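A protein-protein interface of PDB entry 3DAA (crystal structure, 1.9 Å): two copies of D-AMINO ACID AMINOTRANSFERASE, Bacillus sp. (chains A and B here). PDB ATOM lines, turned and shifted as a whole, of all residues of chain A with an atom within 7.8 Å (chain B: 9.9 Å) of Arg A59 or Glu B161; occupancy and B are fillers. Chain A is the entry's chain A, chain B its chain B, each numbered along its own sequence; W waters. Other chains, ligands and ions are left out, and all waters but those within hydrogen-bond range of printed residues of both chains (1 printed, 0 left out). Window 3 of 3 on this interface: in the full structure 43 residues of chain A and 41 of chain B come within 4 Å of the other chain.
OE1 of Gln B157 sits at hydrogen-bond distance from N of Phe A102. The side-chain carboxylate (OE2) of Glu B161 is in salt-bridge range of the guanidinium group (NH2) of Arg A59, at 2.7 Å.
The backbone carbonyl oxygen (O) of Cys B164 lies within hydrogen-bond range of a ring nitrogen (ND1) of His B160. The backbone carbonyl oxygen (O) of Arg A59 is in hydrogen-bond range of the guanidinium group (NH1) of Arg A93 (3.2 Å). The side-chain carboxylate (OE1) of Glu B166 lies within salt-bridge range of the side-chain amino group (NZ) of Lys B156, 2.9 Å away. OD2 of Asp A28 lies within salt-bridge range of NE of Arg A93 (2.8 Å). NE2 of Gln B157 lies within hydrogen-bond range of OE2 of Glu B161.
Asp A28 touches Leu B150. Asp A28 touches Val B153 (OD2 to CG1, 3.96 Å). CG of Lys B156 touches OE1 of Gln A101 (3.8 Å). Gln B157 touches Gln A101. His B160 touches Gln A101 (CD2 to CG, 3.4 Å). Phe A102 touches Val B153 (CE1 to CG1, 3.9 Å).
No residue of chain B comes within 4 Å of Ile A58. Of the printed residues of chain B, Arg A59 touches Glu B161 (2.7 Å). No residue of chain B comes within 4 Å of Ile A60. Pro A109 touches none of the printed residues of chain B. Of the printed residues of chain A, Leu B150 touches Asp A28. Printed residues of chain A within 4 Å of Lys B156: Gln A101. Of the printed residues of chain A, Gln B157 touches Gln A101 and Phe A102. Of chain A, only Arg A59 comes within 4 Å of Glu B161. Lys B162 touches none of the printed residues of chain A.
Of the 19 printed residues of chain B, 6 touch a printed residue of chain A. Printed residues of chain B that touch a printed residue of chain A: Leu B150, Val B153, Lys B156, Gln B157, His B160 and Glu B161. Printed residues of chain A that touch a printed residue of chain B: Asp A28, Arg A59, Gln A101 and Phe A102. Hydrophobic or aromatic side chains of chain A within 4 Å of the printed part of chain B: Phe A102.
No position is printed for both chains.
Water W1 bridges the backbone carbonyl oxygen (O) of Phe A102 and the side-chain amide oxygen (OE1) of Gln B157.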
ATOM      1  N   ASP A  28      -9.327  13.697  16.739  1.00  0.00           N
ATOM      2  CA  ASP A  28      -8.804  13.026  15.544  1.00  0.00           C
ATOM      3  C   ASP A  28      -9.300  13.708  14.268  1.00  0.00           C
ATOM      4  O   ASP A  28     -10.198  13.212  13.579  1.00  0.00           O
ATOM      5  CB  ASP A  28      -9.239  11.544  15.591  1.00  0.00           C
ATOM      6  CG  ASP A  28      -8.530  10.675  14.573  1.00  0.00           C
ATOM      7  OD1 ASP A  28      -7.617  11.157  13.866  1.00  0.00           O
ATOM      8  OD2 ASP A  28      -8.884   9.481  14.499  1.00  0.00           O
ATOM      9  N   VAL A  30      -8.232  17.389  11.384  1.00  0.00           N
ATOM     10  CA  VAL A  30      -7.386  18.521  11.025  1.00  0.00           C
ATOM     11  C   VAL A  30      -8.267  19.691  10.593  1.00  0.00           C
ATOM     12  O   VAL A  30      -9.440  19.486  10.275  1.00  0.00           O
ATOM     13  CB  VAL A  30      -6.412  18.121   9.898  1.00  0.00           C
ATOM     14  CG1 VAL A  30      -5.586  16.933  10.343  1.00  0.00           C
ATOM     15  CG2 VAL A  30      -7.169  17.762   8.624  1.00  0.00           C
ATOM     16  N   TYR A  52      -5.531  19.038   2.945  1.00  0.00           N
ATOM     17  CA  TYR A  52      -5.340  17.687   2.429  1.00  0.00           C
ATOM     18  C   TYR A  52      -4.009  17.082   2.883  1.00  0.00           C
ATOM     19  O   TYR A  52      -3.919  15.872   3.094  1.00  0.00           O
ATOM     20  CB  TYR A  52      -5.467  17.656   0.900  1.00  0.00           C
ATOM     21  CG  TYR A  52      -6.904  17.734   0.409  1.00  0.00           C
ATOM     22  CD1 TYR A  52      -7.687  18.873   0.639  1.00  0.00           C
ATOM     23  CD2 TYR A  52      -7.484  16.668  -0.281  1.00  0.00           C
ATOM     24  CE1 TYR A  52      -9.015  18.945   0.196  1.00  0.00           C
ATOM     25  CE2 TYR A  52      -8.809  16.729  -0.731  1.00  0.00           C
ATOM     26  CZ  TYR A  52      -9.564  17.869  -0.488  1.00  0.00           C
ATOM     27  OH  TYR A  52     -10.869  17.925  -0.923  1.00  0.00           O
ATOM     28  N   ALA A  53      -2.986  17.922   3.045  1.00  0.00           N
ATOM     29  CA  ALA A  53      -1.675  17.458   3.498  1.00  0.00           C
ATOM     30  C   ALA A  53      -1.728  17.024   4.959  1.00  0.00           C
ATOM     31  O   ALA A  53      -1.152  16.001   5.318  1.00  0.00           O
ATOM     32  CB  ALA A  53      -0.623  18.542   3.308  1.00  0.00           C
ATOM     33  N   SER A  54      -2.383  17.821   5.804  1.00  0.00           N
ATOM     34  CA  SER A  54      -2.529  17.492   7.229  1.00  0.00           C
ATOM     35  C   SER A  54      -3.279  16.160   7.333  1.00  0.00           C
ATOM     36  O   SER A  54      -2.923  15.290   8.129  1.00  0.00           O
ATOM     37  CB  SER A  54      -3.331  18.577   7.964  1.00  0.00           C
ATOM     38  OG  SER A  54      -2.649  19.817   8.010  1.00  0.00           O
ATOM     39  N   ALA A  55      -4.333  16.033   6.527  1.00  0.00           N
ATOM     40  CA  ALA A  55      -5.151  14.825   6.460  1.00  0.00           C
ATOM     41  C   ALA A  55      -4.289  13.611   6.096  1.00  0.00           C
ATOM     42  O   ALA A  55      -4.285  12.611   6.810  1.00  0.00           O
ATOM     43  CB  ALA A  55      -6.265  15.011   5.423  1.00  0.00           C
ATOM     44  N   GLU A  56      -3.551  13.706   4.995  1.00  0.00           N
ATOM     45  CA  GLU A  56      -2.680  12.614   4.562  1.00  0.00           C
ATOM     46  C   GLU A  56      -1.688  12.219   5.652  1.00  0.00           C
ATOM     47  O   GLU A  56      -1.359  11.039   5.794  1.00  0.00           O
ATOM     48  CB  GLU A  56      -1.896  13.007   3.307  1.00  0.00           C
ATOM     49  CG  GLU A  56      -2.720  13.178   2.045  1.00  0.00           C
ATOM     50  CD  GLU A  56      -3.342  11.881   1.543  1.00  0.00           C
ATOM     51  OE1 GLU A  56      -2.712  10.808   1.667  1.00  0.00           O
ATOM     52  OE2 GLU A  56      -4.471  11.941   1.012  1.00  0.00           O
ATOM     53  N   LYS A  57      -1.217  13.206   6.420  1.00  0.00           N
ATOM     54  CA  LYS A  57      -0.251  12.957   7.496  1.00  0.00           C
ATOM     55  C   LYS A  57      -0.794  12.079   8.614  1.00  0.00           C
ATOM     56  O   LYS A  57      -0.021  11.443   9.330  1.00  0.00           O
ATOM     57  CB  LYS A  57       0.327  14.265   8.048  1.00  0.00           C
ATOM     58  CG  LYS A  57       1.388  14.898   7.140  1.00  0.00           C
ATOM     59  CD  LYS A  57       1.910  16.225   7.696  1.00  0.00           C
ATOM     60  CE  LYS A  57       3.057  16.782   6.846  1.00  0.00           C
ATOM     61  NZ  LYS A  57       3.677  18.004   7.449  1.00  0.00           N
ATOM     62  N   ILE A  58      -2.111  12.073   8.794  1.00  0.00           N
ATOM     63  CA  ILE A  58      -2.726  11.210   9.794  1.00  0.00           C
ATOM     64  C   ILE A  58      -3.642  10.193   9.101  1.00  0.00           C
ATOM     65  O   ILE A  58      -4.601   9.672   9.685  1.00  0.00           O
ATOM     66  CB  ILE A  58      -3.466  11.984  10.906  1.00  0.00           C
ATOM     67  CG1 ILE A  58      -4.525  12.922  10.328  1.00  0.00           C
ATOM     68  CG2 ILE A  58      -2.456  12.738  11.778  1.00  0.00           C
ATOM     69  CD1 ILE A  58      -5.414  13.542  11.414  1.00  0.00           C
ATOM     70  N   ARG A  59      -3.321   9.937   7.834  1.00  0.00           N
ATOM     71  CA  ARG A  59      -4.016   8.978   6.975  1.00  0.00           C
ATOM     72  C   ARG A  59      -5.548   9.025   6.891  1.00  0.00           C
ATOM     73  O   ARG A  59      -6.221   7.992   6.969  1.00  0.00           O
ATOM     74  CB  ARG A  59      -3.500   7.566   7.274  1.00  0.00           C
ATOM     75  CG  ARG A  59      -2.004   7.447   6.982  1.00  0.00           C
ATOM     76  CD  ARG A  59      -1.311   6.436   7.864  1.00  0.00           C
ATOM     77  NE  ARG A  59      -1.681   5.075   7.511  1.00  0.00           N
ATOM     78  CZ  ARG A  59      -1.533   4.023   8.310  1.00  0.00           C
ATOM     79  NH1 ARG A  59      -1.020   4.159   9.528  1.00  0.00           N
ATOM     80  NH2 ARG A  59      -1.916   2.829   7.891  1.00  0.00           N
ATOM     81  N   ILE A  60      -6.092  10.232   6.762  1.00  0.00           N
ATOM     82  CA  ILE A  60      -7.527  10.411   6.602  1.00  0.00           C
ATOM     83  C   ILE A  60      -7.719  10.719   5.127  1.00  0.00           C
ATOM     84  O   ILE A  60      -7.090  11.630   4.579  1.00  0.00           O
ATOM     85  CB  ILE A  60      -8.099  11.610   7.394  1.00  0.00           C
ATOM     86  CG1 ILE A  60      -8.017  11.361   8.895  1.00  0.00           C
ATOM     87  CG2 ILE A  60      -9.563  11.840   7.004  1.00  0.00           C
ATOM     88  CD1 ILE A  60      -8.652  12.453   9.727  1.00  0.00           C
ATOM     89  N   THR A  61      -8.573   9.945   4.476  1.00  0.00           N
ATOM     90  CA  THR A  61      -8.852  10.160   3.072  1.00  0.00           C
ATOM     91  C   THR A  61     -10.108  10.997   2.922  1.00  0.00           C
ATOM     92  O   THR A  61     -11.220  10.493   3.098  1.00  0.00           O
ATOM     93  CB  THR A  61      -9.027   8.830   2.324  1.00  0.00           C
ATOM     94  OG1 THR A  61      -7.824   8.062   2.439  1.00  0.00           O
ATOM     95  CG2 THR A  61      -9.335   9.077   0.841  1.00  0.00           C
ATOM     96  N   ILE A  62      -9.922  12.284   2.631  1.00  0.00           N
ATOM     97  CA  ILE A  62     -11.044  13.188   2.421  1.00  0.00           C
ATOM     98  C   ILE A  62     -11.854  12.576   1.257  1.00  0.00           C
ATOM     99  O   ILE A  62     -11.304  12.288   0.178  1.00  0.00           O
ATOM    100  CB  ILE A  62     -10.542  14.633   2.132  1.00  0.00           C
ATOM    101  CG1 ILE A  62      -9.747  15.141   3.342  1.00  0.00           C
ATOM    102  CG2 ILE A  62     -11.712  15.581   1.847  1.00  0.00           C
ATOM    103  CD1 ILE A  62      -9.364  16.621   3.295  1.00  0.00           C
ATOM    104  N   ARG A  93     -11.864  11.946  11.267  1.00  0.00           N
ATOM    105  CA  ARG A  93     -11.833  10.614  10.667  1.00  0.00           C
ATOM    106  C   ARG A  93     -13.235  10.012  10.497  1.00  0.00           C
ATOM    107  O   ARG A  93     -13.424   9.100   9.694  1.00  0.00           O
ATOM    108  CB  ARG A  93     -10.953   9.661  11.478  1.00  0.00           C
ATOM    109  CG  ARG A  93     -10.513   8.432  10.674  1.00  0.00           C
ATOM    110  CD  ARG A  93      -9.531   7.557  11.442  1.00  0.00           C
ATOM    111  NE  ARG A  93      -8.412   8.338  11.964  1.00  0.00           N
ATOM    112  CZ  ARG A  93      -7.332   8.674  11.267  1.00  0.00           C
ATOM    113  NH1 ARG A  93      -7.205   8.290  10.004  1.00  0.00           N
ATOM    114  NH2 ARG A  93      -6.394   9.428  11.824  1.00  0.00           N
ATOM    115  N   GLN A 101      -7.547   2.717  17.741  1.00  0.00           N
ATOM    116  CA  GLN A 101      -7.094   2.453  16.376  1.00  0.00           C
ATOM    117  C   GLN A 101      -8.094   2.897  15.309  1.00  0.00           C
ATOM    118  O   GLN A 101      -9.255   3.193  15.615  1.00  0.00           O
ATOM    119  CB  GLN A 101      -6.729   0.970  16.195  1.00  0.00           C
ATOM    120  CG  GLN A 101      -7.908  -0.023  16.123  1.00  0.00           C
ATOM    121  CD  GLN A 101      -8.513  -0.399  17.475  1.00  0.00           C
ATOM    122  OE1 GLN A 101      -8.102   0.086  18.535  1.00  0.00           O
ATOM    123  NE2 GLN A 101      -9.496  -1.285  17.435  1.00  0.00           N
ATOM    124  N   PHE A 102      -7.621   2.970  14.066  1.00  0.00           N
ATOM    125  CA  PHE A 102      -8.444   3.362  12.918  1.00  0.00           C
ATOM    126  C   PHE A 102      -9.612   2.378  12.759  1.00  0.00           C
ATOM    127  O   PHE A 102      -9.445   1.179  12.974  1.00  0.00           O
ATOM    128  CB  PHE A 102      -7.611   3.313  11.624  1.00  0.00           C
ATOM    129  CG  PHE A 102      -6.523   4.375  11.521  1.00  0.00           C
ATOM    130  CD1 PHE A 102      -6.310   5.308  12.534  1.00  0.00           C
ATOM    131  CD2 PHE A 102      -5.707   4.428  10.387  1.00  0.00           C
ATOM    132  CE1 PHE A 102      -5.306   6.279  12.415  1.00  0.00           C
ATOM    133  CE2 PHE A 102      -4.704   5.396  10.259  1.00  0.00           C
ATOM    134  CZ  PHE A 102      -4.503   6.321  11.276  1.00  0.00           C
ATOM    135  N   THR A 106     -13.299   1.186   6.688  1.00  0.00           N
ATOM    136  CA  THR A 106     -13.270   2.610   6.350  1.00  0.00           C
ATOM    137  C   THR A 106     -14.614   3.360   6.432  1.00  0.00           C
ATOM    138  O   THR A 106     -15.520   3.135   5.619  1.00  0.00           O
ATOM    139  CB  THR A 106     -12.661   2.816   4.941  1.00  0.00           C
ATOM    140  OG1 THR A 106     -11.432   2.081   4.836  1.00  0.00           O
ATOM    141  CG2 THR A 106     -12.383   4.297   4.689  1.00  0.00           C
ATOM    142  N   PRO A 109     -15.330  10.331   6.503  1.00  0.00           N
ATOM    143  CA  PRO A 109     -14.854  11.492   7.272  1.00  0.00           C
ATOM    144  C   PRO A 109     -15.913  12.595   7.348  1.00  0.00           C
ATOM    145  O   PRO A 109     -16.604  12.863   6.366  1.00  0.00           O
ATOM    146  CB  PRO A 109     -13.645  11.961   6.464  1.00  0.00           C
ATOM    147  CG  PRO A 109     -13.144  10.709   5.849  1.00  0.00           C
ATOM    148  CD  PRO A 109     -14.418  10.048   5.384  1.00  0.00           C
ATOM    149  N   LYS B 130       1.135  -9.778  22.629  1.00  0.00           N
ATOM    150  CA  LYS B 130       2.349  -9.227  22.020  1.00  0.00           C
ATOM    151  C   LYS B 130       2.275  -7.697  22.069  1.00  0.00           C
ATOM    152  O   LYS B 130       1.209  -7.113  21.875  1.00  0.00           O
ATOM    153  CB  LYS B 130       2.457  -9.636  20.550  1.00  0.00           C
ATOM    154  CG  LYS B 130       2.592 -11.120  20.282  1.00  0.00           C
ATOM    155  CD  LYS B 130       2.254 -11.392  18.824  1.00  0.00           C
ATOM    156  CE  LYS B 130       2.425 -12.850  18.462  1.00  0.00           C
ATOM    157  NZ  LYS B 130       3.857 -13.243  18.432  1.00  0.00           N
ATOM    158  N   THR B 132       4.604  -3.790  21.150  1.00  0.00           N
ATOM    159  CA  THR B 132       5.618  -3.180  20.291  1.00  0.00           C
ATOM    160  C   THR B 132       6.036  -1.828  20.881  1.00  0.00           C
ATOM    161  O   THR B 132       5.205  -1.113  21.444  1.00  0.00           O
ATOM    162  CB  THR B 132       5.093  -3.006  18.825  1.00  0.00           C
ATOM    163  OG1 THR B 132       6.145  -2.523  17.981  1.00  0.00           O
ATOM    164  CG2 THR B 132       3.924  -2.034  18.767  1.00  0.00           C
ATOM    165  N   VAL B 134       7.066   1.997  20.839  1.00  0.00           N
ATOM    166  CA  VAL B 134       6.750   3.161  20.004  1.00  0.00           C
ATOM    167  C   VAL B 134       7.170   4.421  20.762  1.00  0.00           C
ATOM    168  O   VAL B 134       6.883   4.564  21.951  1.00  0.00           O
ATOM    169  CB  VAL B 134       5.226   3.247  19.673  1.00  0.00           C
ATOM    170  CG1 VAL B 134       4.937   4.432  18.768  1.00  0.00           C
ATOM    171  CG2 VAL B 134       4.750   1.967  19.007  1.00  0.00           C
ATOM    172  N   LEU B 150      -4.691  12.240  19.908  1.00  0.00           N
ATOM    173  CA  LEU B 150      -4.183  11.896  18.582  1.00  0.00           C
ATOM    174  C   LEU B 150      -2.875  11.105  18.626  1.00  0.00           C
ATOM    175  O   LEU B 150      -2.613  10.271  17.754  1.00  0.00           O
ATOM    176  CB  LEU B 150      -4.055  13.149  17.697  1.00  0.00           C
ATOM    177  CG  LEU B 150      -3.765  12.944  16.200  1.00  0.00           C
ATOM    178  CD1 LEU B 150      -4.636  11.852  15.596  1.00  0.00           C
ATOM    179  CD2 LEU B 150      -3.975  14.253  15.456  1.00  0.00           C
ATOM    180  N   VAL B 153      -3.825   7.530  19.331  1.00  0.00           N
ATOM    181  CA  VAL B 153      -4.512   6.943  18.176  1.00  0.00           C
ATOM    182  C   VAL B 153      -3.472   6.384  17.194  1.00  0.00           C
ATOM    183  O   VAL B 153      -3.553   5.229  16.766  1.00  0.00           O
ATOM    184  CB  VAL B 153      -5.399   8.001  17.444  1.00  0.00           C
ATOM    185  CG1 VAL B 153      -5.831   7.500  16.057  1.00  0.00           C
ATOM    186  CG2 VAL B 153      -6.617   8.331  18.281  1.00  0.00           C
ATOM    187  N   LEU B 154      -2.486   7.211  16.863  1.00  0.00           N
ATOM    188  CA  LEU B 154      -1.415   6.819  15.942  1.00  0.00           C
ATOM    189  C   LEU B 154      -0.567   5.674  16.503  1.00  0.00           C
ATOM    190  O   LEU B 154      -0.157   4.778  15.751  1.00  0.00           O
ATOM    191  CB  LEU B 154      -0.531   8.025  15.613  1.00  0.00           C
ATOM    192  CG  LEU B 154      -1.256   9.216  14.978  1.00  0.00           C
ATOM    193  CD1 LEU B 154      -0.311  10.390  14.877  1.00  0.00           C
ATOM    194  CD2 LEU B 154      -1.797   8.826  13.611  1.00  0.00           C
ATOM    195  N   ALA B 155      -0.329   5.697  17.817  1.00  0.00           N
ATOM    196  CA  ALA B 155       0.453   4.653  18.484  1.00  0.00           C
ATOM    197  C   ALA B 155      -0.282   3.307  18.500  1.00  0.00           C
ATOM    198  O   ALA B 155       0.315   2.269  18.224  1.00  0.00           O
ATOM    199  CB  ALA B 155       0.814   5.076  19.903  1.00  0.00           C
ATOM    200  N   LYS B 156      -1.575   3.324  18.822  1.00  0.00           N
ATOM    201  CA  LYS B 156      -2.366   2.095  18.855  1.00  0.00           C
ATOM    202  C   LYS B 156      -2.479   1.500  17.446  1.00  0.00           C
ATOM    203  O   LYS B 156      -2.393   0.284  17.270  1.00  0.00           O
ATOM    204  CB  LYS B 156      -3.766   2.371  19.414  1.00  0.00           C
ATOM    205  CG  LYS B 156      -4.621   1.120  19.611  1.00  0.00           C
ATOM    206  CD  LYS B 156      -4.231   0.348  20.868  1.00  0.00           C
ATOM    207  CE  LYS B 156      -4.719   1.065  22.123  1.00  0.00           C
ATOM    208  NZ  LYS B 156      -4.299   0.363  23.367  1.00  0.00           N
ATOM    209  N   GLN B 157      -2.667   2.366  16.450  1.00  0.00           N
ATOM    210  CA  GLN B 157      -2.777   1.927  15.064  1.00  0.00           C
ATOM    211  C   GLN B 157      -1.495   1.209  14.638  1.00  0.00           C
ATOM    212  O   GLN B 157      -1.554   0.147  14.019  1.00  0.00           O
ATOM    213  CB  GLN B 157      -3.073   3.120  14.149  1.00  0.00           C
ATOM    214  CG  GLN B 157      -3.138   2.795  12.651  1.00  0.00           C
ATOM    215  CD  GLN B 157      -4.170   1.722  12.302  1.00  0.00           C
ATOM    216  OE1 GLN B 157      -5.113   1.475  13.058  1.00  0.00           O
ATOM    217  NE2 GLN B 157      -3.989   1.082  11.152  1.00  0.00           N
ATOM    218  N   GLU B 158      -0.338   1.767  14.998  1.00  0.00           N
ATOM    219  CA  GLU B 158       0.939   1.145  14.656  1.00  0.00           C
ATOM    220  C   GLU B 158       1.065  -0.246  15.296  1.00  0.00           C
ATOM    221  O   GLU B 158       1.633  -1.166  14.697  1.00  0.00           O
ATOM    222  CB  GLU B 158       2.116   2.027  15.089  1.00  0.00           C
ATOM    223  CG  GLU B 158       3.473   1.393  14.795  1.00  0.00           C
ATOM    224  CD  GLU B 158       4.650   2.323  15.017  1.00  0.00           C
ATOM    225  OE1 GLU B 158       4.455   3.537  15.195  1.00  0.00           O
ATOM    226  OE2 GLU B 158       5.792   1.833  14.992  1.00  0.00           O
ATOM    227  N   ALA B 159       0.535  -0.392  16.509  1.00  0.00           N
ATOM    228  CA  ALA B 159       0.573  -1.672  17.217  1.00  0.00           C
ATOM    229  C   ALA B 159      -0.270  -2.709  16.469  1.00  0.00           C
ATOM    230  O   ALA B 159       0.225  -3.790  16.137  1.00  0.00           O
ATOM    231  CB  ALA B 159       0.072  -1.508  18.652  1.00  0.00           C
ATOM    232  N   HIS B 160      -1.518  -2.351  16.155  1.00  0.00           N
ATOM    233  CA  HIS B 160      -2.431  -3.247  15.440  1.00  0.00           C
ATOM    234  C   HIS B 160      -1.919  -3.700  14.073  1.00  0.00           C
ATOM    235  O   HIS B 160      -2.121  -4.856  13.687  1.00  0.00           O
ATOM    236  CB  HIS B 160      -3.820  -2.616  15.293  1.00  0.00           C
ATOM    237  CG  HIS B 160      -4.685  -2.774  16.503  1.00  0.00           C
ATOM    238  ND1 HIS B 160      -4.172  -2.917  17.776  1.00  0.00           N
ATOM    239  CD2 HIS B 160      -6.032  -2.805  16.638  1.00  0.00           C
ATOM    240  CE1 HIS B 160      -5.163  -3.026  18.640  1.00  0.00           C
ATOM    241  NE2 HIS B 160      -6.303  -2.962  17.977  1.00  0.00           N
ATOM    242  N   GLU B 161      -1.267  -2.798  13.340  1.00  0.00           N
ATOM    243  CA  GLU B 161      -0.729  -3.143  12.023  1.00  0.00           C
ATOM    244  C   GLU B 161       0.382  -4.176  12.148  1.00  0.00           C
ATOM    245  O   GLU B 161       0.662  -4.908  11.206  1.00  0.00           O
ATOM    246  CB  GLU B 161      -0.191  -1.904  11.314  1.00  0.00           C
ATOM    247  CG  GLU B 161      -1.256  -0.931  10.879  1.00  0.00           C
ATOM    248  CD  GLU B 161      -0.687   0.397  10.452  1.00  0.00           C
ATOM    249  OE1 GLU B 161       0.526   0.622  10.628  1.00  0.00           O
ATOM    250  OE2 GLU B 161      -1.465   1.231   9.958  1.00  0.00           O
ATOM    251  N   LYS B 162       1.025  -4.211  13.314  1.00  0.00           N
ATOM    252  CA  LYS B 162       2.100  -5.160  13.589  1.00  0.00           C
ATOM    253  C   LYS B 162       1.555  -6.419  14.267  1.00  0.00           C
ATOM    254  O   LYS B 162       2.326  -7.282  14.684  1.00  0.00           O
ATOM    255  CB  LYS B 162       3.154  -4.520  14.498  1.00  0.00           C
ATOM    256  CG  LYS B 162       3.924  -3.371  13.885  1.00  0.00           C
ATOM    257  CD  LYS B 162       4.915  -2.801  14.889  1.00  0.00           C
ATOM    258  CE  LYS B 162       5.799  -1.726  14.268  1.00  0.00           C
ATOM    259  NZ  LYS B 162       6.720  -1.131  15.283  1.00  0.00           N
ATOM    260  N   GLY B 163       0.230  -6.508  14.390  1.00  0.00           N
ATOM    261  CA  GLY B 163      -0.388  -7.653  15.040  1.00  0.00           C
ATOM    262  C   GLY B 163      -0.183  -7.665  16.550  1.00  0.00           C
ATOM    263  O   GLY B 163      -0.174  -8.724  17.180  1.00  0.00           O
ATOM    264  N   CYS B 164      -0.033  -6.476  17.127  1.00  0.00           N
ATOM    265  CA  CYS B 164       0.187  -6.317  18.560  1.00  0.00           C
ATOM    266  C   CYS B 164      -1.021  -5.717  19.271  1.00  0.00           C
ATOM    267  O   CYS B 164      -1.734  -4.879  18.727  1.00  0.00           O
ATOM    268  CB  CYS B 164       1.429  -5.454  18.810  1.00  0.00           C
ATOM    269  SG  CYS B 164       2.977  -6.204  18.222  1.00  0.00           S
ATOM    270  N   TYR B 165      -1.223  -6.149  20.509  1.00  0.00           N
ATOM    271  CA  TYR B 165      -2.343  -5.698  21.326  1.00  0.00           C
ATOM    272  C   TYR B 165      -2.145  -4.292  21.869  1.00  0.00           C
ATOM    273  O   TYR B 165      -3.110  -3.536  22.016  1.00  0.00           O
ATOM    274  CB  TYR B 165      -2.554  -6.671  22.495  1.00  0.00           C
ATOM    275  CG  TYR B 165      -3.657  -6.277  23.463  1.00  0.00           C
ATOM    276  CD1 TYR B 165      -5.002  -6.467  23.135  1.00  0.00           C
ATOM    277  CD2 TYR B 165      -3.354  -5.713  24.710  1.00  0.00           C
ATOM    278  CE1 TYR B 165      -6.020  -6.104  24.021  1.00  0.00           C
ATOM    279  CE2 TYR B 165      -4.361  -5.347  25.600  1.00  0.00           C
ATOM    280  CZ  TYR B 165      -5.689  -5.546  25.247  1.00  0.00           C
ATOM    281  OH  TYR B 165      -6.686  -5.176  26.109  1.00  0.00           O
ATOM    282  N   GLU B 166      -0.895  -3.948  22.163  1.00  0.00           N
ATOM    283  CA  GLU B 166      -0.593  -2.646  22.730  1.00  0.00           C
ATOM    284  C   GLU B 166       0.766  -2.070  22.324  1.00  0.00           C
ATOM    285  O   GLU B 166       1.714  -2.802  22.049  1.00  0.00           O
ATOM    286  CB  GLU B 166      -0.691  -2.729  24.274  1.00  0.00           C
ATOM    287  CG  GLU B 166      -0.301  -1.464  25.068  1.00  0.00           C
ATOM    288  CD  GLU B 166      -1.239  -0.298  24.827  1.00  0.00           C
ATOM    289  OE1 GLU B 166      -1.414   0.098  23.654  1.00  0.00           O
ATOM    290  OE2 GLU B 166      -1.809   0.230  25.809  1.00  0.00           O
ATOM    291  N   ALA B 167       0.813  -0.743  22.253  1.00  0.00           N
ATOM    292  CA  ALA B 167       2.031  -0.002  21.956  1.00  0.00           C
ATOM    293  C   ALA B 167       2.590   0.483  23.298  1.00  0.00           C
ATOM    294  O   ALA B 167       1.891   1.172  24.056  1.00  0.00           O
ATOM    295  CB  ALA B 167       1.720   1.194  21.065  1.00  0.00           C
HETATM  296  O   HOH W   1      -7.180  -0.450  12.645  1.00  0.00           O
